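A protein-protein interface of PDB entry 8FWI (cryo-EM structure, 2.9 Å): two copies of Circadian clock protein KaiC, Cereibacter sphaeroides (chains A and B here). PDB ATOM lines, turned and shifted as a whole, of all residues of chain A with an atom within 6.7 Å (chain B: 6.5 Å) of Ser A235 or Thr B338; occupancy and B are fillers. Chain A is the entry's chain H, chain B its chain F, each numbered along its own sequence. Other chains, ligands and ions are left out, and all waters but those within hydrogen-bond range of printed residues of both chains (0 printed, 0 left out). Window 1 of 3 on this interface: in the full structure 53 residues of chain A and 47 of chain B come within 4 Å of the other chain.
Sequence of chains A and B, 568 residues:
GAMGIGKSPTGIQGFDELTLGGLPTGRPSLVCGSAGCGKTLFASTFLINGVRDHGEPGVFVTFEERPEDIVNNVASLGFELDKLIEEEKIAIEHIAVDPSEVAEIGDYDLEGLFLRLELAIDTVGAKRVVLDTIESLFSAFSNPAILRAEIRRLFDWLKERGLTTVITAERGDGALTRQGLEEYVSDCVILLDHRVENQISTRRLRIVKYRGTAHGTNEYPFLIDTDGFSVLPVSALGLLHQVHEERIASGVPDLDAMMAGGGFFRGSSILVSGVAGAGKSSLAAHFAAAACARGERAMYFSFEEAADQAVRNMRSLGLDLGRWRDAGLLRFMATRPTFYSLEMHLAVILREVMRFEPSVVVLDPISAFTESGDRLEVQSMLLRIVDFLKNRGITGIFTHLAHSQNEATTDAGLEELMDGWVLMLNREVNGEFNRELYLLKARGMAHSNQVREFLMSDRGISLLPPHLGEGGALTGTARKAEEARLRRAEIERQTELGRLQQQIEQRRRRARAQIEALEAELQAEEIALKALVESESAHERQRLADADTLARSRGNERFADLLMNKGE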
ATOM      1  N   LEU A  18      -4.311 -27.545  -9.611  1.00  0.00           N
ATOM      2  CA  LEU A  18      -3.572 -26.937  -8.514  1.00  0.00           C
ATOM      3  C   LEU A  18      -4.056 -27.459  -7.166  1.00  0.00           C
ATOM      4  O   LEU A  18      -3.250 -27.708  -6.262  1.00  0.00           O
ATOM      5  CB  LEU A  18      -3.705 -25.418  -8.580  1.00  0.00           C
ATOM      6  CG  LEU A  18      -3.003 -24.736  -9.754  1.00  0.00           C
ATOM      7  CD1 LEU A  18      -3.463 -23.296  -9.885  1.00  0.00           C
ATOM      8  CD2 LEU A  18      -1.496 -24.800  -9.594  1.00  0.00           C
ATOM      9  N   ASN A 218       1.936 -20.684  -5.208  1.00  0.00           N
ATOM     10  CA  ASN A 218       2.376 -19.502  -5.929  1.00  0.00           C
ATOM     11  C   ASN A 218       1.168 -18.699  -6.404  1.00  0.00           C
ATOM     12  O   ASN A 218       0.013 -19.090  -6.219  1.00  0.00           O
ATOM     13  CB  ASN A 218       3.266 -19.898  -7.107  1.00  0.00           C
ATOM     14  CG  ASN A 218       4.515 -20.630  -6.674  1.00  0.00           C
ATOM     15  OD1 ASN A 218       4.913 -20.575  -5.512  1.00  0.00           O
ATOM     16  ND2 ASN A 218       5.147 -21.319  -7.615  1.00  0.00           N
ATOM     17  N   TYR A 220      -0.910 -17.387  -9.568  1.00  0.00           N
ATOM     18  CA  TYR A 220      -1.146 -17.899 -10.915  1.00  0.00           C
ATOM     19  C   TYR A 220      -2.004 -16.928 -11.708  1.00  0.00           C
ATOM     20  O   TYR A 220      -3.223 -16.849 -11.467  1.00  0.00           O
ATOM     21  CB  TYR A 220      -1.816 -19.270 -10.849  1.00  0.00           C
ATOM     22  CG  TYR A 220      -1.007 -20.287 -10.085  1.00  0.00           C
ATOM     23  CD1 TYR A 220       0.095 -20.897 -10.663  1.00  0.00           C
ATOM     24  CD2 TYR A 220      -1.335 -20.630  -8.784  1.00  0.00           C
ATOM     25  CE1 TYR A 220       0.842 -21.824  -9.971  1.00  0.00           C
ATOM     26  CE2 TYR A 220      -0.595 -21.555  -8.083  1.00  0.00           C
ATOM     27  CZ  TYR A 220       0.493 -22.150  -8.681  1.00  0.00           C
ATOM     28  OH  TYR A 220       1.236 -23.073  -7.984  1.00  0.00           O
ATOM     29  N   LEU A 232      -3.782 -21.434 -16.642  1.00  0.00           N
ATOM     30  CA  LEU A 232      -2.786 -22.269 -17.312  1.00  0.00           C
ATOM     31  C   LEU A 232      -1.490 -22.164 -16.518  1.00  0.00           C
ATOM     32  O   LEU A 232      -0.564 -21.439 -16.911  1.00  0.00           O
ATOM     33  CB  LEU A 232      -2.578 -21.846 -18.766  1.00  0.00           C
ATOM     34  CG  LEU A 232      -3.748 -22.098 -19.716  1.00  0.00           C
ATOM     35  CD1 LEU A 232      -3.449 -21.542 -21.098  1.00  0.00           C
ATOM     36  CD2 LEU A 232      -4.061 -23.581 -19.795  1.00  0.00           C
ATOM     37  N   PRO A 233      -1.388 -22.874 -15.396  1.00  0.00           N
ATOM     38  CA  PRO A 233      -0.218 -22.708 -14.528  1.00  0.00           C
ATOM     39  C   PRO A 233       1.060 -23.150 -15.222  1.00  0.00           C
ATOM     40  O   PRO A 233       1.067 -24.095 -16.013  1.00  0.00           O
ATOM     41  CB  PRO A 233      -0.545 -23.594 -13.321  1.00  0.00           C
ATOM     42  CG  PRO A 233      -1.501 -24.602 -13.844  1.00  0.00           C
ATOM     43  CD  PRO A 233      -2.302 -23.916 -14.898  1.00  0.00           C
ATOM     44  N   VAL A 234       2.155 -22.451 -14.913  1.00  0.00           N
ATOM     45  CA  VAL A 234       3.461 -22.816 -15.457  1.00  0.00           C
ATOM     46  C   VAL A 234       4.107 -23.958 -14.695  1.00  0.00           C
ATOM     47  O   VAL A 234       5.095 -24.530 -15.176  1.00  0.00           O
ATOM     48  CB  VAL A 234       4.403 -21.596 -15.458  1.00  0.00           C
ATOM     49  CG1 VAL A 234       4.750 -21.185 -14.038  1.00  0.00           C
ATOM     50  CG2 VAL A 234       5.659 -21.896 -16.252  1.00  0.00           C
ATOM     51  N   SER A 235       3.578 -24.315 -13.525  1.00  0.00           N
ATOM     52  CA  SER A 235       4.121 -25.414 -12.743  1.00  0.00           C
ATOM     53  C   SER A 235       3.633 -26.775 -13.217  1.00  0.00           C
ATOM     54  O   SER A 235       4.132 -27.797 -12.733  1.00  0.00           O
ATOM     55  CB  SER A 235       3.761 -25.233 -11.268  1.00  0.00           C
ATOM     56  OG  SER A 235       4.130 -23.945 -10.808  1.00  0.00           O
ATOM     57  N   ALA A 236       2.677 -26.816 -14.142  1.00  0.00           N
ATOM     58  CA  ALA A 236       2.191 -28.069 -14.697  1.00  0.00           C
ATOM     59  C   ALA A 236       2.991 -28.521 -15.907  1.00  0.00           C
ATOM     60  O   ALA A 236       2.771 -29.634 -16.397  1.00  0.00           O
ATOM     61  CB  ALA A 236       0.716 -27.938 -15.086  1.00  0.00           C
ATOM     62  N   LEU A 237       3.907 -27.693 -16.394  1.00  0.00           N
ATOM     63  CA  LEU A 237       4.736 -28.049 -17.535  1.00  0.00           C
ATOM     64  C   LEU A 237       5.866 -28.952 -17.069  1.00  0.00           C
ATOM     65  O   LEU A 237       6.671 -28.563 -16.217  1.00  0.00           O
ATOM     66  CB  LEU A 237       5.309 -26.799 -18.191  1.00  0.00           C
ATOM     67  CG  LEU A 237       4.345 -25.690 -18.593  1.00  0.00           C
ATOM     68  CD1 LEU A 237       5.145 -24.614 -19.275  1.00  0.00           C
ATOM     69  CD2 LEU A 237       3.224 -26.184 -19.498  1.00  0.00           C
ATOM     70  N   GLY A 238       5.928 -30.159 -17.627  1.00  0.00           N
ATOM     71  CA  GLY A 238       7.017 -31.070 -17.382  1.00  0.00           C
ATOM     72  C   GLY A 238       7.986 -31.124 -18.547  1.00  0.00           C
ATOM     73  O   GLY A 238       7.927 -30.328 -19.486  1.00  0.00           O
ATOM     74  N   SER A 380       7.698 -16.860 -18.875  1.00  0.00           N
ATOM     75  CA  SER A 380       6.679 -17.861 -18.568  1.00  0.00           C
ATOM     76  C   SER A 380       5.761 -18.094 -19.763  1.00  0.00           C
ATOM     77  O   SER A 380       5.481 -19.242 -20.136  1.00  0.00           O
ATOM     78  CB  SER A 380       5.869 -17.426 -17.348  1.00  0.00           C
ATOM     79  OG  SER A 380       6.702 -17.246 -16.218  1.00  0.00           O
ATOM     80  N   LEU A 383       7.710 -19.948 -22.531  1.00  0.00           N
ATOM     81  CA  LEU A 383       7.957 -21.328 -22.132  1.00  0.00           C
ATOM     82  C   LEU A 383       6.702 -22.171 -22.280  1.00  0.00           C
ATOM     83  O   LEU A 383       6.764 -23.316 -22.743  1.00  0.00           O
ATOM     84  CB  LEU A 383       8.459 -21.364 -20.688  1.00  0.00           C
ATOM     85  CG  LEU A 383       8.798 -22.739 -20.112  1.00  0.00           C
ATOM     86  CD1 LEU A 383      10.082 -23.240 -20.722  1.00  0.00           C
ATOM     87  CD2 LEU A 383       8.931 -22.670 -18.605  1.00  0.00           C
ATOM     88  N   THR B 335      13.362 -32.670 -15.008  1.00  0.00           N
ATOM     89  CA  THR B 335      12.324 -31.812 -14.452  1.00  0.00           C
ATOM     90  C   THR B 335      12.685 -30.359 -14.725  1.00  0.00           C
ATOM     91  O   THR B 335      13.840 -29.960 -14.558  1.00  0.00           O
ATOM     92  CB  THR B 335      12.154 -32.025 -12.943  1.00  0.00           C
ATOM     93  OG1 THR B 335      13.374 -31.694 -12.269  1.00  0.00           O
ATOM     94  CG2 THR B 335      11.785 -33.470 -12.632  1.00  0.00           C
ATOM     95  N   ARG B 336      11.694 -29.576 -15.141  1.00  0.00           N
ATOM     96  CA  ARG B 336      11.935 -28.171 -15.419  1.00  0.00           C
ATOM     97  C   ARG B 336      12.223 -27.417 -14.123  1.00  0.00           C
ATOM     98  O   ARG B 336      11.765 -27.814 -13.049  1.00  0.00           O
ATOM     99  CB  ARG B 336      10.734 -27.545 -16.120  1.00  0.00           C
ATOM    100  CG  ARG B 336      10.573 -27.973 -17.559  1.00  0.00           C
ATOM    101  CD  ARG B 336       9.298 -27.432 -18.176  1.00  0.00           C
ATOM    102  NE  ARG B 336       9.061 -27.955 -19.516  1.00  0.00           N
ATOM    103  CZ  ARG B 336       9.594 -27.456 -20.622  1.00  0.00           C
ATOM    104  NH1 ARG B 336      10.432 -26.435 -20.586  1.00  0.00           N
ATOM    105  NH2 ARG B 336       9.281 -27.996 -21.796  1.00  0.00           N
ATOM    106  N   PRO B 337      12.985 -26.323 -14.194  1.00  0.00           N
ATOM    107  CA  PRO B 337      13.256 -25.547 -12.974  1.00  0.00           C
ATOM    108  C   PRO B 337      12.011 -24.955 -12.340  1.00  0.00           C
ATOM    109  O   PRO B 337      12.029 -24.655 -11.141  1.00  0.00           O
ATOM    110  CB  PRO B 337      14.213 -24.448 -13.457  1.00  0.00           C
ATOM    111  CG  PRO B 337      14.749 -24.931 -14.756  1.00  0.00           C
ATOM    112  CD  PRO B 337      13.669 -25.754 -15.366  1.00  0.00           C
ATOM    113  N   THR B 338      10.935 -24.777 -13.102  1.00  0.00           N
ATOM    114  CA  THR B 338       9.708 -24.182 -12.591  1.00  0.00           C
ATOM    115  C   THR B 338       8.730 -25.212 -12.042  1.00  0.00           C
ATOM    116  O   THR B 338       7.648 -24.832 -11.582  1.00  0.00           O
ATOM    117  CB  THR B 338       9.022 -23.371 -13.693  1.00  0.00           C
ATOM    118  OG1 THR B 338       8.974 -24.143 -14.899  1.00  0.00           O
ATOM    119  CG2 THR B 338       9.773 -22.077 -13.953  1.00  0.00           C
ATOM    120  N   PHE B 339       9.079 -26.499 -12.079  1.00  0.00           N
ATOM    121  CA  PHE B 339       8.167 -27.525 -11.585  1.00  0.00           C
ATOM    122  C   PHE B 339       8.066 -27.508 -10.067  1.00  0.00           C
ATOM    123  O   PHE B 339       7.008 -27.831  -9.515  1.00  0.00           O
ATOM    124  CB  PHE B 339       8.624 -28.901 -12.064  1.00  0.00           C
ATOM    125  CG  PHE B 339       7.553 -29.950 -12.005  1.00  0.00           C
ATOM    126  CD1 PHE B 339       6.497 -29.929 -12.897  1.00  0.00           C
ATOM    127  CD2 PHE B 339       7.603 -30.958 -11.059  1.00  0.00           C
ATOM    128  CE1 PHE B 339       5.512 -30.893 -12.846  1.00  0.00           C
ATOM    129  CE2 PHE B 339       6.621 -31.922 -11.004  1.00  0.00           C
ATOM    130  CZ  PHE B 339       5.575 -31.890 -11.898  1.00  0.00           C
ATOM    131  N   TYR B 340       9.143 -27.138  -9.379  1.00  0.00           N
ATOM    132  CA  TYR B 340       9.201 -27.156  -7.929  1.00  0.00           C
ATOM    133  C   TYR B 340       9.708 -25.815  -7.420  1.00  0.00           C
ATOM    134  O   TYR B 340      10.142 -24.951  -8.188  1.00  0.00           O
ATOM    135  CB  TYR B 340      10.121 -28.273  -7.416  1.00  0.00           C
ATOM    136  CG  TYR B 340       9.608 -29.674  -7.636  1.00  0.00           C
ATOM    137  CD1 TYR B 340       8.282 -30.000  -7.393  1.00  0.00           C
ATOM    138  CD2 TYR B 340      10.457 -30.679  -8.076  1.00  0.00           C
ATOM    139  CE1 TYR B 340       7.816 -31.283  -7.588  1.00  0.00           C
ATOM    140  CE2 TYR B 340      10.001 -31.962  -8.275  1.00  0.00           C
ATOM    141  CZ  TYR B 340       8.680 -32.261  -8.030  1.00  0.00           C
ATOM    142  OH  TYR B 340       8.225 -33.544  -8.228  1.00  0.00           O
ATOM    143  N   SER B 341       9.643 -25.652  -6.105  1.00  0.00           N
ATOM    144  CA  SER B 341      10.290 -24.543  -5.428  1.00  0.00           C
ATOM    145  C   SER B 341      11.714 -24.934  -5.055  1.00  0.00           C
ATOM    146  O   SER B 341      12.060 -26.114  -4.972  1.00  0.00           O
ATOM    147  CB  SER B 341       9.505 -24.138  -4.181  1.00  0.00           C
ATOM    148  OG  SER B 341       9.410 -25.214  -3.265  1.00  0.00           O
ATOM    149  N   HIS B 345      13.096 -28.753  -4.794  1.00  0.00           N
ATOM    150  CA  HIS B 345      14.113 -29.269  -5.705  1.00  0.00           C
ATOM    151  C   HIS B 345      15.221 -29.963  -4.922  1.00  0.00           C
ATOM    152  O   HIS B 345      15.571 -31.119  -5.193  1.00  0.00           O
ATOM    153  CB  HIS B 345      14.683 -28.126  -6.545  1.00  0.00           C
ATOM    154  CG  HIS B 345      14.020 -27.954  -7.876  1.00  0.00           C
ATOM    155  ND1 HIS B 345      13.835 -28.997  -8.758  1.00  0.00           N
ATOM    156  CD2 HIS B 345      13.517 -26.855  -8.484  1.00  0.00           C
ATOM    157  CE1 HIS B 345      13.235 -28.551  -9.846  1.00  0.00           C
ATOM    158  NE2 HIS B 345      13.031 -27.254  -9.705  1.00  0.00           N
ATOM    159  N   PHE B 369      18.754 -22.457 -12.848  1.00  0.00           N
ATOM    160  CA  PHE B 369      17.988 -21.979 -11.705  1.00  0.00           C
ATOM    161  C   PHE B 369      18.181 -20.488 -11.429  1.00  0.00           C
ATOM    162  O   PHE B 369      17.764 -20.012 -10.370  1.00  0.00           O
ATOM    163  CB  PHE B 369      18.369 -22.770 -10.449  1.00  0.00           C
ATOM    164  CG  PHE B 369      18.002 -24.228 -10.501  1.00  0.00           C
ATOM    165  CD1 PHE B 369      16.681 -24.633 -10.418  1.00  0.00           C
ATOM    166  CD2 PHE B 369      18.986 -25.198 -10.604  1.00  0.00           C
ATOM    167  CE1 PHE B 369      16.350 -25.974 -10.454  1.00  0.00           C
ATOM    168  CE2 PHE B 369      18.658 -26.537 -10.639  1.00  0.00           C
ATOM    169  CZ  PHE B 369      17.340 -26.924 -10.564  1.00  0.00           C
ATOM    170  N   SER B 372      14.893 -18.698 -10.977  1.00  0.00           N
ATOM    171  CA  SER B 372      13.965 -19.344 -10.057  1.00  0.00           C
ATOM    172  C   SER B 372      13.962 -18.703  -8.675  1.00  0.00           C
ATOM    173  O   SER B 372      13.180 -19.121  -7.816  1.00  0.00           O
ATOM    174  CB  SER B 372      14.301 -20.832  -9.928  1.00  0.00           C
ATOM    175  OG  SER B 372      14.087 -21.498 -11.161  1.00  0.00           O
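The guanidinium group of Arg B336 lies within hydrogen-bond range of the backbone carbonyl oxygen of Gly A238 (2.6 Å).
Among the printed residues, pairs that only touch across the chains: Ser A235 with Phe B339 (3.2 Å), Leu A383 with Arg B336 (3.2 Å), Leu A237 with Arg B336 (3.5 Å), Leu A237 with Phe B339 (3.6 Å), Ser A235 with Thr B338 (3.7 Å), Val A234 with Thr B338 (3.9 Å) and Leu A383 with Thr B338 (3.99 Å).
Ser A235 touches just these residues of chain B: Thr B338 (3.7 Å) and Phe B339 (3.2 Å). Printed residues of chain B within 4 Å of Leu A237: Arg B336 and Phe B339. Of the printed residues of chain A, Arg B336 touches Leu A237, Gly A238 and Leu A383. Of the printed residues of chain A, Thr B338 touches Val A234, Ser A235 and Leu A383. His B345 touches none of the printed residues of chain A. The nearest printed residue of chain A that does not touch Thr B338 is Leu A237 (5.2 Å). The nearest printed residue of chain A that does not touch Phe B339 is Ala A236 (4.6 Å).
Of the 12 printed residues of chain A, 5 touch a printed residue of chain B.
No position is printed for both chains. Of the 8 pairs that touch across the chains among the printed residues, none has its exchanged pair printed and touching as well.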
